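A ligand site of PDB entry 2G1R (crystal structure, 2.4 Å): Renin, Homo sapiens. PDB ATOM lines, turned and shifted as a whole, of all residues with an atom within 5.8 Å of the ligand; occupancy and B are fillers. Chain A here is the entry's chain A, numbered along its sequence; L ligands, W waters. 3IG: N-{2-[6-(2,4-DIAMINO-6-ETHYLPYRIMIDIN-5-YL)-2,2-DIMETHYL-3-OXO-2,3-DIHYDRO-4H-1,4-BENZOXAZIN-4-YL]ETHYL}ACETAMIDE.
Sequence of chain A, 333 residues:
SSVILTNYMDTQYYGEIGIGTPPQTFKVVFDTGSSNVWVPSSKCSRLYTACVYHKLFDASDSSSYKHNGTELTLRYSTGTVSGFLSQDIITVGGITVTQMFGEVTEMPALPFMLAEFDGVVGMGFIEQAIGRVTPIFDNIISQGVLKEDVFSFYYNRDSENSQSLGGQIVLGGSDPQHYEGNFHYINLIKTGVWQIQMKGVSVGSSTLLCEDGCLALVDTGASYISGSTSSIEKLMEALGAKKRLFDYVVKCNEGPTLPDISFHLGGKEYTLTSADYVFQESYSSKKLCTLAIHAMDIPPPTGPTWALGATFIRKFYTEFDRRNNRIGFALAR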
ATOM      1  N   THR A  11      26.158  -4.544   3.920  1.00  0.00           N
ATOM      2  CA  THR A  11      26.696  -5.097   5.156  1.00  0.00           C
ATOM      3  C   THR A  11      26.140  -6.479   5.468  1.00  0.00           C
ATOM      4  O   THR A  11      26.734  -7.219   6.262  1.00  0.00           O
ATOM      5  CB  THR A  11      26.426  -4.184   6.356  1.00  0.00           C
ATOM      6  OG1 THR A  11      25.012  -3.977   6.493  1.00  0.00           O
ATOM      7  CG2 THR A  11      27.132  -2.837   6.174  1.00  0.00           C
ATOM      8  N   GLN A  12      25.004  -6.819   4.861  1.00  0.00           N
ATOM      9  CA  GLN A  12      24.386  -8.113   5.090  1.00  0.00           C
ATOM     10  C   GLN A  12      24.083  -8.858   3.796  1.00  0.00           C
ATOM     11  O   GLN A  12      23.382  -8.346   2.915  1.00  0.00           O
ATOM     12  CB  GLN A  12      23.097  -7.944   5.920  1.00  0.00           C
ATOM     13  CG  GLN A  12      23.347  -7.559   7.372  1.00  0.00           C
ATOM     14  CD  GLN A  12      22.064  -7.321   8.176  1.00  0.00           C
ATOM     15  OE1 GLN A  12      21.169  -8.157   8.197  1.00  0.00           O
ATOM     16  NE2 GLN A  12      22.005  -6.180   8.854  1.00  0.00           N
ATOM     17  N   TYR A  13      24.638 -10.067   3.675  1.00  0.00           N
ATOM     18  CA  TYR A  13      24.439 -10.900   2.494  1.00  0.00           C
ATOM     19  C   TYR A  13      23.888 -12.234   2.973  1.00  0.00           C
ATOM     20  O   TYR A  13      24.556 -12.962   3.701  1.00  0.00           O
ATOM     21  CB  TYR A  13      25.749 -11.129   1.724  1.00  0.00           C
ATOM     22  CG  TYR A  13      26.320  -9.863   1.104  1.00  0.00           C
ATOM     23  CD1 TYR A  13      26.987  -8.921   1.875  1.00  0.00           C
ATOM     24  CD2 TYR A  13      26.187  -9.617  -0.251  1.00  0.00           C
ATOM     25  CE1 TYR A  13      27.505  -7.760   1.313  1.00  0.00           C
ATOM     26  CE2 TYR A  13      26.706  -8.449  -0.840  1.00  0.00           C
ATOM     27  CZ  TYR A  13      27.364  -7.535  -0.041  1.00  0.00           C
ATOM     28  OH  TYR A  13      27.880  -6.397  -0.594  1.00  0.00           O
ATOM     29  N   TYR A  14      22.662 -12.551   2.572  1.00  0.00           N
ATOM     30  CA  TYR A  14      22.036 -13.786   3.014  1.00  0.00           C
ATOM     31  C   TYR A  14      21.221 -14.458   1.933  1.00  0.00           C
ATOM     32  O   TYR A  14      20.738 -13.814   1.003  1.00  0.00           O
ATOM     33  CB  TYR A  14      21.136 -13.492   4.210  1.00  0.00           C
ATOM     34  CG  TYR A  14      20.137 -12.390   3.953  1.00  0.00           C
ATOM     35  CD1 TYR A  14      20.420 -11.068   4.292  1.00  0.00           C
ATOM     36  CD2 TYR A  14      18.907 -12.651   3.347  1.00  0.00           C
ATOM     37  CE1 TYR A  14      19.505 -10.059   4.050  1.00  0.00           C
ATOM     38  CE2 TYR A  14      17.999 -11.646   3.082  1.00  0.00           C
ATOM     39  CZ  TYR A  14      18.294 -10.353   3.444  1.00  0.00           C
ATOM     40  OH  TYR A  14      17.378  -9.341   3.232  1.00  0.00           O
ATOM     41  N   VAL A  29      23.145 -16.163   6.551  1.00  0.00           N
ATOM     42  CA  VAL A  29      24.419 -15.676   6.026  1.00  0.00           C
ATOM     43  C   VAL A  29      25.343 -16.891   5.906  1.00  0.00           C
ATOM     44  O   VAL A  29      25.358 -17.739   6.789  1.00  0.00           O
ATOM     45  CB  VAL A  29      25.070 -14.678   7.016  1.00  0.00           C
ATOM     46  CG1 VAL A  29      26.425 -14.240   6.496  1.00  0.00           C
ATOM     47  CG2 VAL A  29      24.164 -13.475   7.213  1.00  0.00           C
ATOM     48  N   ASP A  31      28.754 -18.068   6.243  1.00  0.00           N
ATOM     49  CA  ASP A  31      29.916 -17.622   6.989  1.00  0.00           C
ATOM     50  C   ASP A  31      31.180 -18.501   7.041  1.00  0.00           C
ATOM     51  O   ASP A  31      31.225 -19.485   7.765  1.00  0.00           O
ATOM     52  CB  ASP A  31      29.397 -17.371   8.405  1.00  0.00           C
ATOM     53  CG  ASP A  31      30.447 -16.911   9.362  1.00  0.00           C
ATOM     54  OD1 ASP A  31      30.221 -17.082  10.572  1.00  0.00           O
ATOM     55  OD2 ASP A  31      31.481 -16.369   8.926  1.00  0.00           O
ATOM     56  N   THR A  32      32.212 -18.113   6.287  1.00  0.00           N
ATOM     57  CA  THR A  32      33.457 -18.879   6.308  1.00  0.00           C
ATOM     58  C   THR A  32      34.181 -18.648   7.628  1.00  0.00           C
ATOM     59  O   THR A  32      35.172 -19.312   7.913  1.00  0.00           O
ATOM     60  CB  THR A  32      34.416 -18.484   5.157  1.00  0.00           C
ATOM     61  OG1 THR A  32      34.625 -17.068   5.159  1.00  0.00           O
ATOM     62  CG2 THR A  32      33.852 -18.940   3.823  1.00  0.00           C
ATOM     63  N   GLY A  33      33.669 -17.725   8.423  1.00  0.00           N
ATOM     64  CA  GLY A  33      34.272 -17.415   9.713  1.00  0.00           C
ATOM     65  C   GLY A  33      33.790 -18.245  10.891  1.00  0.00           C
ATOM     66  O   GLY A  33      34.341 -18.137  11.978  1.00  0.00           O
ATOM     67  N   SER A  34      32.753 -19.055  10.699  1.00  0.00           N
ATOM     68  CA  SER A  34      32.257 -19.920  11.779  1.00  0.00           C
ATOM     69  C   SER A  34      31.984 -21.305  11.168  1.00  0.00           C
ATOM     70  O   SER A  34      32.071 -21.464   9.952  1.00  0.00           O
ATOM     71  CB  SER A  34      30.971 -19.343  12.401  1.00  0.00           C
ATOM     72  OG  SER A  34      29.896 -19.274  11.487  1.00  0.00           O
ATOM     73  N   TYR A  76      30.411 -14.854  18.361  1.00  0.00           N
ATOM     74  CA  TYR A  76      30.955 -14.141  17.214  1.00  0.00           C
ATOM     75  C   TYR A  76      31.606 -12.861  17.730  1.00  0.00           C
ATOM     76  O   TYR A  76      31.417 -12.482  18.888  1.00  0.00           O
ATOM     77  CB  TYR A  76      29.859 -13.833  16.187  1.00  0.00           C
ATOM     78  CG  TYR A  76      29.091 -15.051  15.704  1.00  0.00           C
ATOM     79  CD1 TYR A  76      27.884 -15.398  16.270  1.00  0.00           C
ATOM     80  CD2 TYR A  76      29.590 -15.863  14.689  1.00  0.00           C
ATOM     81  CE1 TYR A  76      27.191 -16.526  15.859  1.00  0.00           C
ATOM     82  CE2 TYR A  76      28.913 -16.989  14.264  1.00  0.00           C
ATOM     83  CZ  TYR A  76      27.699 -17.311  14.858  1.00  0.00           C
ATOM     84  OH  TYR A  76      27.000 -18.431  14.456  1.00  0.00           O
ATOM     85  N   SER A  77      32.397 -12.216  16.892  1.00  0.00           N
ATOM     86  CA  SER A  77      33.090 -10.997  17.276  1.00  0.00           C
ATOM     87  C   SER A  77      32.131  -9.866  17.642  1.00  0.00           C
ATOM     88  O   SER A  77      32.486  -8.946  18.377  1.00  0.00           O
ATOM     89  CB  SER A  77      33.977 -10.526  16.133  1.00  0.00           C
ATOM     90  OG  SER A  77      33.174 -10.233  15.007  1.00  0.00           O
ATOM     91  N   THR A  78      30.914  -9.932  17.118  1.00  0.00           N
ATOM     92  CA  THR A  78      29.960  -8.875  17.370  1.00  0.00           C
ATOM     93  C   THR A  78      28.693  -9.298  18.081  1.00  0.00           C
ATOM     94  O   THR A  78      27.721  -8.546  18.120  1.00  0.00           O
ATOM     95  CB  THR A  78      29.577  -8.179  16.062  1.00  0.00           C
ATOM     96  OG1 THR A  78      29.075  -9.153  15.137  1.00  0.00           O
ATOM     97  CG2 THR A  78      30.790  -7.492  15.462  1.00  0.00           C
ATOM     98  N   GLY A  79      28.696 -10.500  18.659  1.00  0.00           N
ATOM     99  CA  GLY A  79      27.512 -10.954  19.351  1.00  0.00           C
ATOM    100  C   GLY A  79      27.538 -12.434  19.644  1.00  0.00           C
ATOM    101  O   GLY A  79      28.362 -13.179  19.109  1.00  0.00           O
ATOM    102  N   PRO A 111      23.091  -7.497  18.816  1.00  0.00           N
ATOM    103  CA  PRO A 111      22.697  -6.836  17.565  1.00  0.00           C
ATOM    104  C   PRO A 111      21.613  -7.502  16.728  1.00  0.00           C
ATOM    105  O   PRO A 111      21.272  -7.006  15.656  1.00  0.00           O
ATOM    106  CB  PRO A 111      23.990  -6.833  16.789  1.00  0.00           C
ATOM    107  CG  PRO A 111      24.439  -8.271  17.048  1.00  0.00           C
ATOM    108  CD  PRO A 111      24.220  -8.419  18.557  1.00  0.00           C
ATOM    109  N   PHE A 112      21.045  -8.611  17.185  1.00  0.00           N
ATOM    110  CA  PHE A 112      20.110  -9.290  16.316  1.00  0.00           C
ATOM    111  C   PHE A 112      18.836  -8.589  15.887  1.00  0.00           C
ATOM    112  O   PHE A 112      18.185  -9.019  14.944  1.00  0.00           O
ATOM    113  CB  PHE A 112      19.866 -10.697  16.834  1.00  0.00           C
ATOM    114  CG  PHE A 112      21.127 -11.528  16.862  1.00  0.00           C
ATOM    115  CD1 PHE A 112      21.830 -11.713  18.034  1.00  0.00           C
ATOM    116  CD2 PHE A 112      21.687 -11.988  15.678  1.00  0.00           C
ATOM    117  CE1 PHE A 112      23.066 -12.346  18.025  1.00  0.00           C
ATOM    118  CE2 PHE A 112      22.909 -12.617  15.655  1.00  0.00           C
ATOM    119  CZ  PHE A 112      23.599 -12.791  16.829  1.00  0.00           C
ATOM    120  N   LEU A 114      18.956  -5.907  14.548  1.00  0.00           N
ATOM    121  CA  LEU A 114      19.400  -5.205  13.350  1.00  0.00           C
ATOM    122  C   LEU A 114      19.681  -6.149  12.186  1.00  0.00           C
ATOM    123  O   LEU A 114      20.037  -5.717  11.095  1.00  0.00           O
ATOM    124  CB  LEU A 114      20.654  -4.392  13.633  1.00  0.00           C
ATOM    125  CG  LEU A 114      20.541  -3.394  14.782  1.00  0.00           C
ATOM    126  CD1 LEU A 114      21.773  -2.521  14.766  1.00  0.00           C
ATOM    127  CD2 LEU A 114      19.277  -2.547  14.620  1.00  0.00           C
ATOM    128  N   ALA A 115      19.509  -7.446  12.430  1.00  0.00           N
ATOM    129  CA  ALA A 115      19.753  -8.453  11.394  1.00  0.00           C
ATOM    130  C   ALA A 115      18.557  -8.668  10.488  1.00  0.00           C
ATOM    131  O   ALA A 115      17.440  -8.896  10.935  1.00  0.00           O
ATOM    132  CB  ALA A 115      20.135  -9.775  12.054  1.00  0.00           C
ATOM    133  N   GLU A 116      18.807  -8.596   9.179  1.00  0.00           N
ATOM    134  CA  GLU A 116      17.753  -8.833   8.201  1.00  0.00           C
ATOM    135  C   GLU A 116      17.610 -10.352   8.102  1.00  0.00           C
ATOM    136  O   GLU A 116      16.543 -10.865   7.812  1.00  0.00           O
ATOM    137  CB  GLU A 116      18.156  -8.280   6.836  1.00  0.00           C
ATOM    138  CG  GLU A 116      17.705  -6.871   6.569  1.00  0.00           C
ATOM    139  CD  GLU A 116      16.206  -6.772   6.396  1.00  0.00           C
ATOM    140  OE1 GLU A 116      15.625  -7.717   5.811  1.00  0.00           O
ATOM    141  OE2 GLU A 116      15.604  -5.768   6.835  1.00  0.00           O
ATOM    142  N   PHE A 117      18.697 -11.064   8.350  1.00  0.00           N
ATOM    143  CA  PHE A 117      18.694 -12.509   8.285  1.00  0.00           C
ATOM    144  C   PHE A 117      18.184 -13.099   9.583  1.00  0.00           C
ATOM    145  O   PHE A 117      18.109 -12.399  10.597  1.00  0.00           O
ATOM    146  CB  PHE A 117      20.108 -13.030   8.043  1.00  0.00           C
ATOM    147  CG  PHE A 117      21.126 -12.521   9.018  1.00  0.00           C
ATOM    148  CD1 PHE A 117      21.772 -11.316   8.803  1.00  0.00           C
ATOM    149  CD2 PHE A 117      21.433 -13.250  10.159  1.00  0.00           C
ATOM    150  CE1 PHE A 117      22.704 -10.843   9.706  1.00  0.00           C
ATOM    151  CE2 PHE A 117      22.366 -12.777  11.062  1.00  0.00           C
ATOM    152  CZ  PHE A 117      23.004 -11.580  10.837  1.00  0.00           C
ATOM    153  N   VAL A 120      22.450 -18.387  10.566  1.00  0.00           N
ATOM    154  CA  VAL A 120      23.759 -18.481   9.955  1.00  0.00           C
ATOM    155  C   VAL A 120      24.130 -19.901   9.542  1.00  0.00           C
ATOM    156  O   VAL A 120      23.836 -20.865  10.240  1.00  0.00           O
ATOM    157  CB  VAL A 120      24.828 -17.954  10.930  1.00  0.00           C
ATOM    158  CG1 VAL A 120      26.222 -18.061  10.305  1.00  0.00           C
ATOM    159  CG2 VAL A 120      24.515 -16.535  11.331  1.00  0.00           C
ATOM    160  N   TYR A 155      29.882 -11.162  -3.986  1.00  0.00           N
ATOM    161  CA  TYR A 155      29.129 -10.145  -3.244  1.00  0.00           C
ATOM    162  C   TYR A 155      29.096  -8.894  -4.117  1.00  0.00           C
ATOM    163  O   TYR A 155      30.110  -8.221  -4.263  1.00  0.00           O
ATOM    164  CB  TYR A 155      29.815  -9.766  -1.924  1.00  0.00           C
ATOM    165  CG  TYR A 155      29.560 -10.699  -0.769  1.00  0.00           C
ATOM    166  CD1 TYR A 155      30.213 -10.508   0.448  1.00  0.00           C
ATOM    167  CD2 TYR A 155      28.693 -11.770  -0.882  1.00  0.00           C
ATOM    168  CE1 TYR A 155      30.009 -11.358   1.510  1.00  0.00           C
ATOM    169  CE2 TYR A 155      28.474 -12.628   0.178  1.00  0.00           C
ATOM    170  CZ  TYR A 155      29.143 -12.422   1.370  1.00  0.00           C
ATOM    171  OH  TYR A 155      28.947 -13.274   2.440  1.00  0.00           O
ATOM    172  N   ASP A 219      36.852 -14.008   5.745  1.00  0.00           N
ATOM    173  CA  ASP A 219      35.561 -14.215   6.394  1.00  0.00           C
ATOM    174  C   ASP A 219      34.327 -13.654   5.697  1.00  0.00           C
ATOM    175  O   ASP A 219      34.011 -12.469   5.809  1.00  0.00           O
ATOM    176  CB  ASP A 219      35.707 -13.625   7.801  1.00  0.00           C
ATOM    177  CG  ASP A 219      34.530 -13.923   8.681  1.00  0.00           C
ATOM    178  OD1 ASP A 219      34.567 -13.465   9.835  1.00  0.00           O
ATOM    179  OD2 ASP A 219      33.584 -14.592   8.209  1.00  0.00           O
ATOM    180  N   THR A 220      33.607 -14.514   4.989  1.00  0.00           N
ATOM    181  CA  THR A 220      32.390 -14.103   4.267  1.00  0.00           C
ATOM    182  C   THR A 220      31.275 -13.657   5.222  1.00  0.00           C
ATOM    183  O   THR A 220      30.307 -13.042   4.801  1.00  0.00           O
ATOM    184  CB  THR A 220      31.836 -15.259   3.416  1.00  0.00           C
ATOM    185  OG1 THR A 220      31.416 -16.322   4.287  1.00  0.00           O
ATOM    186  CG2 THR A 220      32.903 -15.776   2.470  1.00  0.00           C
ATOM    187  N   GLY A 221      31.433 -13.977   6.500  1.00  0.00           N
ATOM    188  CA  GLY A 221      30.425 -13.605   7.469  1.00  0.00           C
ATOM    189  C   GLY A 221      30.661 -12.247   8.109  1.00  0.00           C
ATOM    190  O   GLY A 221      29.804 -11.761   8.845  1.00  0.00           O
ATOM    191  N   ALA A 222      31.810 -11.626   7.817  1.00  0.00           N
ATOM    192  CA  ALA A 222      32.115 -10.313   8.375  1.00  0.00           C
ATOM    193  C   ALA A 222      31.769  -9.205   7.382  1.00  0.00           C
ATOM    194  O   ALA A 222      32.067  -9.286   6.205  1.00  0.00           O
ATOM    195  CB  ALA A 222      33.587 -10.231   8.733  1.00  0.00           C
ATOM    196  N   SER A 223      31.112  -8.156   7.859  1.00  0.00           N
ATOM    197  CA  SER A 223      30.718  -7.074   6.975  1.00  0.00           C
ATOM    198  C   SER A 223      31.915  -6.285   6.466  1.00  0.00           C
ATOM    199  O   SER A 223      31.939  -5.867   5.318  1.00  0.00           O
ATOM    200  CB  SER A 223      29.786  -6.100   7.689  1.00  0.00           C
ATOM    201  OG  SER A 223      28.622  -6.771   8.136  1.00  0.00           O
ATOM    202  N   ALA A 310      33.205  -8.692   3.599  1.00  0.00           N
ATOM    203  CA  ALA A 310      32.446  -8.210   2.451  1.00  0.00           C
ATOM    204  C   ALA A 310      33.111  -7.045   1.722  1.00  0.00           C
ATOM    205  O   ALA A 310      33.082  -6.976   0.494  1.00  0.00           O
ATOM    206  CB  ALA A 310      31.030  -7.820   2.878  1.00  0.00           C
HETATM  207  C1  3IG L   1      30.572 -12.292  12.667  1.00  0.00           C
HETATM  208  N1  3IG L   1      31.670 -13.009  12.307  1.00  0.00           N
HETATM  209  C2  3IG L   1      31.432 -14.196  11.727  1.00  0.00           C
HETATM  210  N2  3IG L   1      30.208 -14.702  11.489  1.00  0.00           N
HETATM  211  C3  3IG L   1      29.102 -14.002  11.837  1.00  0.00           C
HETATM  212  C4  3IG L   1      29.233 -12.722  12.451  1.00  0.00           C
HETATM  213  N3  3IG L   1      30.817 -11.103  13.241  1.00  0.00           N
HETATM  214  N4  3IG L   1      32.471 -14.934  11.343  1.00  0.00           N
HETATM  215  C5  3IG L   1      27.763 -14.654  11.519  1.00  0.00           C
HETATM  216  C6  3IG L   1      27.270 -14.308  10.114  1.00  0.00           C
HETATM  217  C7  3IG L   1      27.348 -11.900  14.022  1.00  0.00           C
HETATM  218  C8  3IG L   1      26.248 -11.004  14.217  1.00  0.00           C
HETATM  219  C9  3IG L   1      25.881 -10.084  13.196  1.00  0.00           C
HETATM  220  C10 3IG L   1      26.623 -10.040  11.979  1.00  0.00           C
HETATM  221  C11 3IG L   1      27.692 -10.958  11.835  1.00  0.00           C
HETATM  222  C12 3IG L   1      28.068 -11.859  12.824  1.00  0.00           C
HETATM  223  O3  3IG L   1      24.791  -9.235  13.409  1.00  0.00           O
HETATM  224  C14 3IG L   1      24.673  -8.046  12.595  1.00  0.00           C
HETATM  225  C15 3IG L   1      25.318  -8.152  11.150  1.00  0.00           C
HETATM  226  N5  3IG L   1      26.255  -9.146  10.936  1.00  0.00           N
HETATM  227  C16 3IG L   1      26.903  -9.180   9.569  1.00  0.00           C
HETATM  228  C17 3IG L   1      26.526 -10.424   8.733  1.00  0.00           C
HETATM  229  N6  3IG L   1      27.468 -10.598   7.621  1.00  0.00           N
HETATM  230  C13 3IG L   1      27.063 -10.642   6.331  1.00  0.00           C
HETATM  231  C19 3IG L   1      28.199 -10.827   5.329  1.00  0.00           C
HETATM  232  C21 3IG L   1      25.332  -6.856  13.329  1.00  0.00           C
HETATM  233  C20 3IG L   1      23.172  -7.773  12.468  1.00  0.00           C
HETATM  234  O4  3IG L   1      24.980  -7.350  10.290  1.00  0.00           O
HETATM  235  O1  3IG L   1      25.897 -10.534   5.957  1.00  0.00           O
HETATM  236  O   HOH W   1      32.989 -16.361  14.112  1.00  0.00           O
HETATM  237  O   HOH W   2      33.313 -13.693  14.449  1.00  0.00           O
HETATM  238  O   HOH W   3      24.480  -4.732   9.548  1.00  0.00           O
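The backbone carbonyl oxygen (O) of Thr 11 lies close to an oxygen (O1) of the ligand, 3.4 Å away. Gln 12 touches the ligand (CA to O1, 3.0 Å). Val 29 touches the ligand. Gly 33 touches the ligand. CD2 of Tyr 76 touches C3 of the ligand (3.4 Å). Pro 111 touches the ligand. Phe 112 touches the ligand. Leu 114 touches the ligand (C to C20, 3.9 Å). Ala 115 touches the ligand. Phe 117 touches the ligand. Val 120 touches the ligand (CG2 to C6, 3.7 Å). Tyr 155 touches the ligand. Thr 220 touches the ligand (O to C19, 3.1 Å). Ser 223 touches the ligand (OG to C16, 3.3 Å).
Water W3 lies within hydrogen-bond range of an oxygen (O4) of the ligand (2.8 Å), the side-chain amide nitrogen of Gln 12 (3.0 Å) and the side-chain hydroxyl of Thr 11 (3.2 Å). Water W2 lies within hydrogen-bond range of N1 of the ligand (2.8 Å) and N of Ser 77 (3.0 Å). Water W1 lies within hydrogen-bond range of O of Gly 33 (3.1 Å) and N4 of the ligand (3.2 Å).
The backbone carbonyl oxygen of Thr 220 is in hydrogen-bond range of the side-chain hydroxyl of Tyr 155 (2.7 Å). The side-chain amide nitrogen (NE2) of Gln 12 sits at hydrogen-bond distance from the backbone carbonyl oxygen (O) of Leu 114 (3.0 Å). N of Gly 33 lies within hydrogen-bond range of OD2 of Asp 31 (2.6 Å). The backbone NH of Gly 221 sits close to the side-chain carboxylate of Asp 31, 3.4 Å away. The side-chain carboxylate (OD1) of Asp 31 sits close to the backbone NH (N) of Ser 34. N of Thr 220 lies within hydrogen-bond range of OG1 of Thr 32, at 2.8 Å. N of Gly 221 lies within hydrogen-bond range of OD2 of Asp 219 (2.8 Å). The backbone NH (N) of Glu 116 lies within hydrogen-bond range of the side-chain amide oxygen (OE1) of Gln 12.
The side-chain hydroxyl (OG) of Ser 77 sits at hydrogen-bond distance from a nitrogen (N3) of the ligand, 3.1 Å away. The backbone NH of Tyr 13 lies within hydrogen-bond range of an oxygen (O1) of the ligand, at 2.6 Å. OD1 of Asp 219 sits at hydrogen-bond distance from N4 of the ligand. N2 of the ligand lies within hydrogen-bond range of OD1 of Asp 31. OG1 of Thr 78 sits at hydrogen-bond distance from N3 of the ligand. O of Gly 221 lies within hydrogen-bond range of N6 of the ligand, 2.9 Å away.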
